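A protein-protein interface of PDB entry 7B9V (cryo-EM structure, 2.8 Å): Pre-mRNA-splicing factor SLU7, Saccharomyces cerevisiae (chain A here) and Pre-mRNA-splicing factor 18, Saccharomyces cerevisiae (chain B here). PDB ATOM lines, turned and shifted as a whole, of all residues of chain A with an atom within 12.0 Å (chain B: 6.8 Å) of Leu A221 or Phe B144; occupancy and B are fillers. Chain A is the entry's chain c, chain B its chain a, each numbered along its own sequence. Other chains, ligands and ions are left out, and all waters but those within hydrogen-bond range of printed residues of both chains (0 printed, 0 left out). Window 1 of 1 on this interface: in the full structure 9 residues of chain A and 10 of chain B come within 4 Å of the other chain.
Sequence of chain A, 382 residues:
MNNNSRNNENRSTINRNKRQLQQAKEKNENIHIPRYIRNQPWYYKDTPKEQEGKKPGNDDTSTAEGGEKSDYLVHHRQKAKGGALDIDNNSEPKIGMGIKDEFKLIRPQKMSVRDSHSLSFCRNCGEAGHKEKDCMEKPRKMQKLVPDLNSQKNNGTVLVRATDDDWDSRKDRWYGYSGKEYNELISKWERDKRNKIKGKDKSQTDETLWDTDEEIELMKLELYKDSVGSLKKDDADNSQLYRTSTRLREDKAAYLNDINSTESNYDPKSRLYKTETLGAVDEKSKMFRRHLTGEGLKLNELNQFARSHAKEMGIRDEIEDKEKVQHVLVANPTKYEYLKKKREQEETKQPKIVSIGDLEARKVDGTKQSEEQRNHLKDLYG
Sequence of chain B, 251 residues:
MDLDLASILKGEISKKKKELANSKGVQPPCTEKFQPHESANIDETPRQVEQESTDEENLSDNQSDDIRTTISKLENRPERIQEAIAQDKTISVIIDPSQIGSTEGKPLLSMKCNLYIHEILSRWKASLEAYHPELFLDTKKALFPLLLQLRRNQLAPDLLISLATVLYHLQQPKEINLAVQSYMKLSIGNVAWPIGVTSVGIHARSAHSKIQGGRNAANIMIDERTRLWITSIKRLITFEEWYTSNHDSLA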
ATOM      1  N   ILE A 216      24.733  12.651  29.788  1.00  0.00           N
ATOM      2  CA  ILE A 216      23.299  12.398  29.848  1.00  0.00           C
ATOM      3  C   ILE A 216      22.891  11.441  28.688  1.00  0.00           C
ATOM      4  O   ILE A 216      21.880  11.608  28.002  1.00  0.00           O
ATOM      5  CB  ILE A 216      22.477  13.751  29.978  1.00  0.00           C
ATOM      6  CG1 ILE A 216      21.018  13.496  30.426  1.00  0.00           C
ATOM      7  CG2 ILE A 216      22.615  14.685  28.750  1.00  0.00           C
ATOM      8  CD1 ILE A 216      20.892  12.836  31.794  1.00  0.00           C
ATOM      9  N   GLU A 217      23.736  10.415  28.446  1.00  0.00           N
ATOM     10  CA  GLU A 217      23.516   9.400  27.398  1.00  0.00           C
ATOM     11  C   GLU A 217      22.258   8.543  27.604  1.00  0.00           C
ATOM     12  O   GLU A 217      21.917   7.741  26.710  1.00  0.00           O
ATOM     13  CB  GLU A 217      24.757   8.504  27.271  1.00  0.00           C
ATOM     14  CG  GLU A 217      26.103   9.250  27.168  1.00  0.00           C
ATOM     15  CD  GLU A 217      26.112  10.440  26.191  1.00  0.00           C
ATOM     16  OE1 GLU A 217      25.545  10.351  25.076  1.00  0.00           O
ATOM     17  OE2 GLU A 217      26.688  11.489  26.545  1.00  0.00           O
ATOM     18  N   LEU A 218      21.617   8.669  28.780  1.00  0.00           N
ATOM     19  CA  LEU A 218      20.230   8.274  29.011  1.00  0.00           C
ATOM     20  C   LEU A 218      19.332   8.748  27.874  1.00  0.00           C
ATOM     21  O   LEU A 218      18.616   7.945  27.277  1.00  0.00           O
ATOM     22  CB  LEU A 218      19.743   8.836  30.353  1.00  0.00           C
ATOM     23  CG  LEU A 218      18.262   8.717  30.728  1.00  0.00           C
ATOM     24  CD1 LEU A 218      17.844   7.278  30.804  1.00  0.00           C
ATOM     25  CD2 LEU A 218      17.955   9.399  32.055  1.00  0.00           C
ATOM     26  N   MET A 219      19.425  10.041  27.513  1.00  0.00           N
ATOM     27  CA  MET A 219      18.614  10.609  26.430  1.00  0.00           C
ATOM     28  C   MET A 219      18.917   9.969  25.075  1.00  0.00           C
ATOM     29  O   MET A 219      17.990   9.714  24.303  1.00  0.00           O
ATOM     30  CB  MET A 219      18.798  12.128  26.361  1.00  0.00           C
ATOM     31  CG  MET A 219      17.798  12.826  25.427  1.00  0.00           C
ATOM     32  SD  MET A 219      16.056  12.578  25.839  1.00  0.00           S
ATOM     33  CE  MET A 219      15.869  13.582  27.309  1.00  0.00           C
ATOM     34  N   LYS A 220      20.194   9.699  24.778  1.00  0.00           N
ATOM     35  CA  LYS A 220      20.609   9.061  23.520  1.00  0.00           C
ATOM     36  C   LYS A 220      19.981   7.675  23.362  1.00  0.00           C
ATOM     37  O   LYS A 220      19.400   7.356  22.320  1.00  0.00           O
ATOM     38  CB  LYS A 220      22.136   8.979  23.426  1.00  0.00           C
ATOM     39  CG  LYS A 220      22.652   8.342  22.122  1.00  0.00           C
ATOM     40  CD  LYS A 220      24.175   8.178  22.099  1.00  0.00           C
ATOM     41  CE  LYS A 220      24.891   9.513  21.928  1.00  0.00           C
ATOM     42  NZ  LYS A 220      26.290   9.466  22.442  1.00  0.00           N
ATOM     43  N   LEU A 221      20.089   6.843  24.397  1.00  0.00           N
ATOM     44  CA  LEU A 221      19.558   5.476  24.342  1.00  0.00           C
ATOM     45  C   LEU A 221      18.023   5.416  24.464  1.00  0.00           C
ATOM     46  O   LEU A 221      17.406   4.524  23.869  1.00  0.00           O
ATOM     47  CB  LEU A 221      20.246   4.592  25.386  1.00  0.00           C
ATOM     48  CG  LEU A 221      19.979   3.084  25.267  1.00  0.00           C
ATOM     49  CD1 LEU A 221      20.485   2.538  23.934  1.00  0.00           C
ATOM     50  CD2 LEU A 221      20.647   2.348  26.383  1.00  0.00           C
ATOM     51  N   GLU A 222      17.389   6.334  25.211  1.00  0.00           N
ATOM     52  CA  GLU A 222      15.917   6.397  25.272  1.00  0.00           C
ATOM     53  C   GLU A 222      15.249   6.728  23.931  1.00  0.00           C
ATOM     54  O   GLU A 222      14.224   6.120  23.601  1.00  0.00           O
ATOM     55  CB  GLU A 222      15.441   7.399  26.329  1.00  0.00           C
ATOM     56  CG  GLU A 222      15.620   7.002  27.800  1.00  0.00           C
ATOM     57  CD  GLU A 222      14.536   6.107  28.370  1.00  0.00           C
ATOM     58  OE1 GLU A 222      14.078   5.157  27.699  1.00  0.00           O
ATOM     59  OE2 GLU A 222      14.152   6.353  29.534  1.00  0.00           O
ATOM     60  N   LEU A 223      15.777   7.693  23.162  1.00  0.00           N
ATOM     61  CA  LEU A 223      15.121   8.198  21.941  1.00  0.00           C
ATOM     62  C   LEU A 223      14.959   7.157  20.822  1.00  0.00           C
ATOM     63  O   LEU A 223      14.193   7.407  19.884  1.00  0.00           O
ATOM     64  CB  LEU A 223      15.867   9.418  21.393  1.00  0.00           C
ATOM     65  CG  LEU A 223      15.710  10.702  22.208  1.00  0.00           C
ATOM     66  CD1 LEU A 223      16.775  11.717  21.833  1.00  0.00           C
ATOM     67  CD2 LEU A 223      14.336  11.291  22.002  1.00  0.00           C
ATOM     68  N   TYR A 224      15.649   6.010  20.894  1.00  0.00           N
ATOM     69  CA  TYR A 224      15.355   4.874  20.015  1.00  0.00           C
ATOM     70  C   TYR A 224      13.958   4.292  20.254  1.00  0.00           C
ATOM     71  O   TYR A 224      13.431   3.602  19.373  1.00  0.00           O
ATOM     72  CB  TYR A 224      16.357   3.735  20.248  1.00  0.00           C
ATOM     73  CG  TYR A 224      17.792   3.956  19.804  1.00  0.00           C
ATOM     74  CD1 TYR A 224      18.672   4.689  20.595  1.00  0.00           C
ATOM     75  CD2 TYR A 224      18.283   3.364  18.639  1.00  0.00           C
ATOM     76  CE1 TYR A 224      19.992   4.880  20.212  1.00  0.00           C
ATOM     77  CE2 TYR A 224      19.607   3.547  18.249  1.00  0.00           C
ATOM     78  CZ  TYR A 224      20.452   4.304  19.041  1.00  0.00           C
ATOM     79  OH  TYR A 224      21.759   4.499  18.666  1.00  0.00           O
ATOM     80  N   LYS A 225      13.358   4.527  21.433  1.00  0.00           N
ATOM     81  CA  LYS A 225      12.182   3.794  21.905  1.00  0.00           C
ATOM     82  C   LYS A 225      11.059   4.684  22.451  1.00  0.00           C
ATOM     83  O   LYS A 225       9.920   4.584  21.982  1.00  0.00           O
ATOM     84  CB  LYS A 225      12.604   2.789  22.982  1.00  0.00           C
ATOM     85  CG  LYS A 225      13.468   1.638  22.473  1.00  0.00           C
ATOM     86  CD  LYS A 225      14.213   0.962  23.610  1.00  0.00           C
ATOM     87  CE  LYS A 225      15.077  -0.180  23.097  1.00  0.00           C
ATOM     88  NZ  LYS A 225      16.012  -0.672  24.141  1.00  0.00           N
ATOM     89  N   ASP A 226      11.344   5.556  23.429  1.00  0.00           N
ATOM     90  CA  ASP A 226      10.325   6.073  24.347  1.00  0.00           C
ATOM     91  C   ASP A 226      10.792   7.381  24.982  1.00  0.00           C
ATOM     92  O   ASP A 226      11.918   7.836  24.760  1.00  0.00           O
ATOM     93  CB  ASP A 226       9.979   5.055  25.448  1.00  0.00           C
ATOM     94  CG  ASP A 226       9.050   3.952  24.975  1.00  0.00           C
ATOM     95  OD1 ASP A 226       7.916   4.262  24.563  1.00  0.00           O
ATOM     96  OD2 ASP A 226       9.480   2.779  24.980  1.00  0.00           O
ATOM     97  N   SER A 227       9.874   8.000  25.743  1.00  0.00           N
ATOM     98  CA  SER A 227      10.164   9.130  26.634  1.00  0.00           C
ATOM     99  C   SER A 227      11.251   8.823  27.664  1.00  0.00           C
ATOM    100  O   SER A 227      11.460   7.674  28.065  1.00  0.00           O
ATOM    101  CB  SER A 227       8.886   9.574  27.352  1.00  0.00           C
ATOM    102  OG  SER A 227       9.138  10.644  28.249  1.00  0.00           O
ATOM    103  N   VAL A 228      11.932   9.889  28.110  1.00  0.00           N
ATOM    104  CA  VAL A 228      12.793   9.826  29.289  1.00  0.00           C
ATOM    105  C   VAL A 228      11.999   9.501  30.561  1.00  0.00           C
ATOM    106  O   VAL A 228      10.838   9.903  30.731  1.00  0.00           O
ATOM    107  CB  VAL A 228      13.621  11.125  29.400  1.00  0.00           C
ATOM    108  CG1 VAL A 228      12.785  12.348  29.790  1.00  0.00           C
ATOM    109  CG2 VAL A 228      14.843  10.961  30.329  1.00  0.00           C
ATOM    110  N   GLY A 229      12.624   8.713  31.441  1.00  0.00           N
ATOM    111  CA  GLY A 229      12.095   8.376  32.750  1.00  0.00           C
ATOM    112  C   GLY A 229      11.945   6.884  32.974  1.00  0.00           C
ATOM    113  O   GLY A 229      11.138   6.221  32.312  1.00  0.00           O
ATOM    114  N   SER A 230      12.709   6.351  33.923  1.00  0.00           N
ATOM    115  CA  SER A 230      12.818   4.909  34.128  1.00  0.00           C
ATOM    116  C   SER A 230      11.629   4.320  34.888  1.00  0.00           C
ATOM    117  O   SER A 230      11.397   3.109  34.860  1.00  0.00           O
ATOM    118  CB  SER A 230      14.129   4.579  34.855  1.00  0.00           C
ATOM    119  OG  SER A 230      14.163   5.146  36.155  1.00  0.00           O
ATOM    120  N   ILE B  81      23.424  12.366  17.958  1.00  0.00           N
ATOM    121  CA  ILE B  81      22.432  11.292  17.787  1.00  0.00           C
ATOM    122  C   ILE B  81      22.257  10.941  16.303  1.00  0.00           C
ATOM    123  O   ILE B  81      22.135   9.756  15.940  1.00  0.00           O
ATOM    124  CB  ILE B  81      21.098  11.671  18.479  1.00  0.00           C
ATOM    125  CG1 ILE B  81      21.261  11.605  19.997  1.00  0.00           C
ATOM    126  CG2 ILE B  81      19.931  10.771  18.078  1.00  0.00           C
ATOM    127  CD1 ILE B  81      20.317  12.497  20.758  1.00  0.00           C
ATOM    128  N   ASN B 114      24.676  -5.176  20.273  1.00  0.00           N
ATOM    129  CA  ASN B 114      23.703  -4.106  20.503  1.00  0.00           C
ATOM    130  C   ASN B 114      22.758  -3.953  19.315  1.00  0.00           C
ATOM    131  O   ASN B 114      21.530  -3.882  19.486  1.00  0.00           O
ATOM    132  CB  ASN B 114      24.462  -2.799  20.795  1.00  0.00           C
ATOM    133  CG  ASN B 114      23.548  -1.570  20.970  1.00  0.00           C
ATOM    134  OD1 ASN B 114      23.057  -0.979  20.003  1.00  0.00           O
ATOM    135  ND2 ASN B 114      23.335  -1.179  22.221  1.00  0.00           N
ATOM    136  N   HIS B 118      18.726  -4.777  18.974  1.00  0.00           N
ATOM    137  CA  HIS B 118      17.822  -3.740  18.458  1.00  0.00           C
ATOM    138  C   HIS B 118      16.977  -4.247  17.297  1.00  0.00           C
ATOM    139  O   HIS B 118      15.795  -3.901  17.183  1.00  0.00           O
ATOM    140  CB  HIS B 118      18.597  -2.494  17.984  1.00  0.00           C
ATOM    141  CG  HIS B 118      18.842  -1.464  19.049  1.00  0.00           C
ATOM    142  ND1 HIS B 118      17.808  -0.783  19.661  1.00  0.00           N
ATOM    143  CD2 HIS B 118      19.987  -0.909  19.522  1.00  0.00           C
ATOM    144  CE1 HIS B 118      18.304   0.084  20.517  1.00  0.00           C
ATOM    145  NE2 HIS B 118      19.627   0.031  20.450  1.00  0.00           N
ATOM    146  N   THR B 139      10.207  -5.558  28.854  1.00  0.00           N
ATOM    147  CA  THR B 139      11.417  -6.122  28.265  1.00  0.00           C
ATOM    148  C   THR B 139      12.349  -5.016  27.774  1.00  0.00           C
ATOM    149  O   THR B 139      13.570  -5.106  27.959  1.00  0.00           O
ATOM    150  CB  THR B 139      11.033  -7.077  27.128  1.00  0.00           C
ATOM    151  OG1 THR B 139      10.184  -8.108  27.649  1.00  0.00           O
ATOM    152  CG2 THR B 139      12.251  -7.756  26.523  1.00  0.00           C
ATOM    153  N   LYS B 140      11.784  -3.977  27.124  1.00  0.00           N
ATOM    154  CA  LYS B 140      12.566  -2.818  26.678  1.00  0.00           C
ATOM    155  C   LYS B 140      13.226  -2.098  27.850  1.00  0.00           C
ATOM    156  O   LYS B 140      14.420  -1.738  27.788  1.00  0.00           O
ATOM    157  CB  LYS B 140      11.697  -1.831  25.885  1.00  0.00           C
ATOM    158  CG  LYS B 140      11.412  -2.229  24.437  1.00  0.00           C
ATOM    159  CD  LYS B 140      10.694  -1.111  23.668  1.00  0.00           C
ATOM    160  CE  LYS B 140       9.275  -0.857  24.162  1.00  0.00           C
ATOM    161  NZ  LYS B 140       8.722   0.416  23.610  1.00  0.00           N
ATOM    162  N   LYS B 141      12.467  -1.943  28.951  1.00  0.00           N
ATOM    163  CA  LYS B 141      13.004  -1.347  30.177  1.00  0.00           C
ATOM    164  C   LYS B 141      14.126  -2.200  30.759  1.00  0.00           C
ATOM    165  O   LYS B 141      15.165  -1.677  31.182  1.00  0.00           O
ATOM    166  CB  LYS B 141      11.886  -1.178  31.211  1.00  0.00           C
ATOM    167  CG  LYS B 141      10.899  -0.053  30.930  1.00  0.00           C
ATOM    168  CD  LYS B 141      10.202   0.398  32.214  1.00  0.00           C
ATOM    169  CE  LYS B 141       9.228  -0.646  32.754  1.00  0.00           C
ATOM    170  NZ  LYS B 141       7.902  -0.581  32.078  1.00  0.00           N
ATOM    171  N   ALA B 142      13.907  -3.517  30.830  1.00  0.00           N
ATOM    172  CA  ALA B 142      14.872  -4.428  31.433  1.00  0.00           C
ATOM    173  C   ALA B 142      16.136  -4.538  30.580  1.00  0.00           C
ATOM    174  O   ALA B 142      17.225  -4.768  31.120  1.00  0.00           O
ATOM    175  CB  ALA B 142      14.230  -5.788  31.680  1.00  0.00           C
ATOM    176  N   LEU B 143      16.016  -4.381  29.253  1.00  0.00           N
ATOM    177  CA  LEU B 143      17.182  -4.460  28.383  1.00  0.00           C
ATOM    178  C   LEU B 143      17.883  -3.128  28.205  1.00  0.00           C
ATOM    179  O   LEU B 143      18.867  -3.096  27.464  1.00  0.00           O
ATOM    180  CB  LEU B 143      16.840  -5.000  27.001  1.00  0.00           C
ATOM    181  CG  LEU B 143      16.424  -6.450  26.908  1.00  0.00           C
ATOM    182  CD1 LEU B 143      15.754  -6.745  25.597  1.00  0.00           C
ATOM    183  CD2 LEU B 143      17.707  -7.257  27.011  1.00  0.00           C
ATOM    184  N   PHE B 144      17.337  -2.038  28.769  1.00  0.00           N
ATOM    185  CA  PHE B 144      18.028  -0.743  28.759  1.00  0.00           C
ATOM    186  C   PHE B 144      19.464  -0.825  29.308  1.00  0.00           C
ATOM    187  O   PHE B 144      20.374  -0.340  28.611  1.00  0.00           O
ATOM    188  CB  PHE B 144      17.174   0.368  29.426  1.00  0.00           C
ATOM    189  CG  PHE B 144      17.883   1.738  29.551  1.00  0.00           C
ATOM    190  CD1 PHE B 144      18.740   2.049  30.630  1.00  0.00           C
ATOM    191  CD2 PHE B 144      17.709   2.691  28.560  1.00  0.00           C
ATOM    192  CE1 PHE B 144      19.384   3.257  30.703  1.00  0.00           C
ATOM    193  CE2 PHE B 144      18.350   3.923  28.648  1.00  0.00           C
ATOM    194  CZ  PHE B 144      19.196   4.187  29.705  1.00  0.00           C
ATOM    195  N   PRO B 145      19.747  -1.362  30.528  1.00  0.00           N
ATOM    196  CA  PRO B 145      21.137  -1.291  31.035  1.00  0.00           C
ATOM    197  C   PRO B 145      22.134  -2.156  30.286  1.00  0.00           C
ATOM    198  O   PRO B 145      23.320  -1.794  30.260  1.00  0.00           O
ATOM    199  CB  PRO B 145      21.018  -1.737  32.491  1.00  0.00           C
ATOM    200  CG  PRO B 145      19.836  -2.508  32.552  1.00  0.00           C
ATOM    201  CD  PRO B 145      18.886  -1.918  31.607  1.00  0.00           C
ATOM    202  N   LEU B 146      21.710  -3.304  29.754  1.00  0.00           N
ATOM    203  CA  LEU B 146      22.595  -4.113  28.917  1.00  0.00           C
ATOM    204  C   LEU B 146      23.031  -3.328  27.685  1.00  0.00           C
ATOM    205  O   LEU B 146      24.212  -3.330  27.337  1.00  0.00           O
ATOM    206  CB  LEU B 146      21.880  -5.398  28.493  1.00  0.00           C
ATOM    207  CG  LEU B 146      22.549  -6.252  27.411  1.00  0.00           C
ATOM    208  CD1 LEU B 146      23.862  -6.849  27.892  1.00  0.00           C
ATOM    209  CD2 LEU B 146      21.609  -7.335  26.900  1.00  0.00           C
ATOM    210  N   LEU B 147      22.088  -2.668  27.012  1.00  0.00           N
ATOM    211  CA  LEU B 147      22.378  -1.950  25.769  1.00  0.00           C
ATOM    212  C   LEU B 147      23.275  -0.729  26.019  1.00  0.00           C
ATOM    213  O   LEU B 147      24.163  -0.431  25.211  1.00  0.00           O
ATOM    214  CB  LEU B 147      21.071  -1.580  25.065  1.00  0.00           C
ATOM    215  CG  LEU B 147      20.339  -2.824  24.528  1.00  0.00           C
ATOM    216  CD1 LEU B 147      18.900  -2.527  24.141  1.00  0.00           C
ATOM    217  CD2 LEU B 147      21.068  -3.452  23.352  1.00  0.00           C
ATOM    218  N   LEU B 148      23.067  -0.031  27.147  1.00  0.00           N
ATOM    219  CA  LEU B 148      23.978   1.035  27.594  1.00  0.00           C
ATOM    220  C   LEU B 148      25.368   0.505  27.928  1.00  0.00           C
ATOM    221  O   LEU B 148      26.375   1.137  27.576  1.00  0.00           O
ATOM    222  CB  LEU B 148      23.397   1.780  28.798  1.00  0.00           C
ATOM    223  CG  LEU B 148      24.169   3.007  29.293  1.00  0.00           C
ATOM    224  CD1 LEU B 148      24.290   4.042  28.190  1.00  0.00           C
ATOM    225  CD2 LEU B 148      23.468   3.622  30.498  1.00  0.00           C
ATOM    226  N   GLN B 149      25.447  -0.627  28.638  1.00  0.00           N
ATOM    227  CA  GLN B 149      26.740  -1.202  29.016  1.00  0.00           C
ATOM    228  C   GLN B 149      27.504  -1.690  27.788  1.00  0.00           C
ATOM    229  O   GLN B 149      28.736  -1.586  27.740  1.00  0.00           O
ATOM    230  CB  GLN B 149      26.516  -2.340  30.016  1.00  0.00           C
ATOM    231  CG  GLN B 149      27.765  -2.858  30.705  1.00  0.00           C
ATOM    232  CD  GLN B 149      27.437  -3.806  31.840  1.00  0.00           C
ATOM    233  OE1 GLN B 149      26.277  -4.164  32.048  1.00  0.00           O
ATOM    234  NE2 GLN B 149      28.458  -4.223  32.581  1.00  0.00           N
ATOM    235  N   ARG B 151      27.070  -0.344  24.769  1.00  0.00           N
ATOM    236  CA  ARG B 151      27.379   0.879  24.023  1.00  0.00           C
ATOM    237  C   ARG B 151      28.654   1.559  24.526  1.00  0.00           C
ATOM    238  O   ARG B 151      29.352   2.221  23.749  1.00  0.00           O
ATOM    239  CB  ARG B 151      26.203   1.859  24.085  1.00  0.00           C
ATOM    240  CG  ARG B 151      26.162   2.873  22.936  1.00  0.00           C
ATOM    241  CD  ARG B 151      25.596   2.301  21.641  1.00  0.00           C
ATOM    242  NE  ARG B 151      25.586   3.289  20.561  1.00  0.00           N
ATOM    243  CZ  ARG B 151      25.047   3.101  19.364  1.00  0.00           C
ATOM    244  NH1 ARG B 151      24.314   2.025  19.097  1.00  0.00           N
ATOM    245  NH2 ARG B 151      25.217   4.031  18.420  1.00  0.00           N
ATOM    246  N   ARG B 225      19.853  -6.026  38.293  1.00  0.00           N
ATOM    247  CA  ARG B 225      19.857  -5.519  36.920  1.00  0.00           C
ATOM    248  C   ARG B 225      20.389  -6.565  35.936  1.00  0.00           C
ATOM    249  O   ARG B 225      19.843  -6.718  34.827  1.00  0.00           O
ATOM    250  CB  ARG B 225      20.689  -4.233  36.853  1.00  0.00           C
ATOM    251  CG  ARG B 225      20.163  -3.114  37.762  1.00  0.00           C
ATOM    252  CD  ARG B 225      21.169  -1.995  38.026  1.00  0.00           C
ATOM    253  NE  ARG B 225      21.369  -1.137  36.861  1.00  0.00           N
ATOM    254  CZ  ARG B 225      22.501  -1.025  36.180  1.00  0.00           C
ATOM    255  NH1 ARG B 225      23.583  -1.703  36.521  1.00  0.00           N
ATOM    256  NH2 ARG B 225      22.550  -0.201  35.138  1.00  0.00           N
ATOM    257  N   TRP B 229      18.205  -8.318  32.781  1.00  0.00           N
ATOM    258  CA  TRP B 229      18.515  -8.298  31.348  1.00  0.00           C
ATOM    259  C   TRP B 229      18.815  -9.702  30.830  1.00  0.00           C
ATOM    260  O   TRP B 229      18.577  -9.984  29.650  1.00  0.00           O
ATOM    261  CB  TRP B 229      19.629  -7.278  31.020  1.00  0.00           C
ATOM    262  CG  TRP B 229      21.077  -7.514  31.448  1.00  0.00           C
ATOM    263  CD1 TRP B 229      21.762  -6.767  32.358  1.00  0.00           C
ATOM    264  CD2 TRP B 229      22.051  -8.411  30.868  1.00  0.00           C
ATOM    265  NE1 TRP B 229      23.056  -7.204  32.466  1.00  0.00           N
ATOM    266  CE2 TRP B 229      23.265  -8.205  31.557  1.00  0.00           C
ATOM    267  CE3 TRP B 229      22.007  -9.394  29.871  1.00  0.00           C
ATOM    268  CZ2 TRP B 229      24.418  -8.939  31.285  1.00  0.00           C
ATOM    269  CZ3 TRP B 229      23.157 -10.121  29.599  1.00  0.00           C
ATOM    270  CH2 TRP B 229      24.345  -9.892  30.307  1.00  0.00           C
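NH2 of Arg B151 lies within hydrogen-bond range of OH of Tyr A224, at 3.5 Å.
The side-chain carboxylate (OD2) of Asp A226 is in salt-bridge range of the side-chain amino group (NZ) of Lys B140, 2.8 Å away.
OD1 of Asn B114 lies within hydrogen-bond range of NH1 of Arg B151.
The backbone carbonyl oxygen (O) of Leu B147 sits at hydrogen-bond distance from the side-chain amide nitrogen (ND2) of Asn B114 (3.2 Å).
Among the printed residues, merely in contact across the chains: Lys A225 with Leu B147, Leu A221 with Leu B148, Leu A221 with Phe B144, Leu A218 with Phe B144, Tyr A224 with His B118, Leu A223 with Ile B81 and Ser A230 with Lys B141.
Of the printed residues of chain B, Leu A218 touches Phe B144.
Of chain B, only Phe B144 and Leu B148 come within 4 Å of Leu A221.
Of the printed residues of chain B, Ser A230 touches Lys B141.
Printed residues of chain A within 4 Å of Phe B144: Leu A218 and Leu A221.
Pro B145 touches none of the printed residues of chain A.
Of chain A, only Lys A225 (3.4 Å) comes within 4 Å of Leu B147.
Printed residues of chain A within 4 Å of Leu B148: Leu A221.
The nearest residue of chain B that does not touch Leu A221 is Leu B147 (4.1 Å).
The nearest residue of chain A that does not touch Phe B144 is Glu A222 (4.2 Å).
The nearest printed residue of chain B that does not touch Leu A218 is Leu B148 (5.4 Å).
Of the 15 printed residues of chain A, 7 touch a printed residue of chain B.
Printed residues of chain A that touch a printed residue of chain B: Leu A218, Leu A221, Leu A223, Tyr A224, Lys A225, Asp A226 and Ser A230.
Hydrophobic or aromatic side chains of chain A that line the printed part of chain B: Leu A218, Leu A221, Leu A223 and Tyr A224.
Among the printed residues, 9 pairs touch across the chains.
Among the printed residues, Asp or Glu carboxylates within 4 Å of a Lys or Arg side-chain nitrogen of the other chain: Asp A226 with Lys B140 (2.8 Å).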
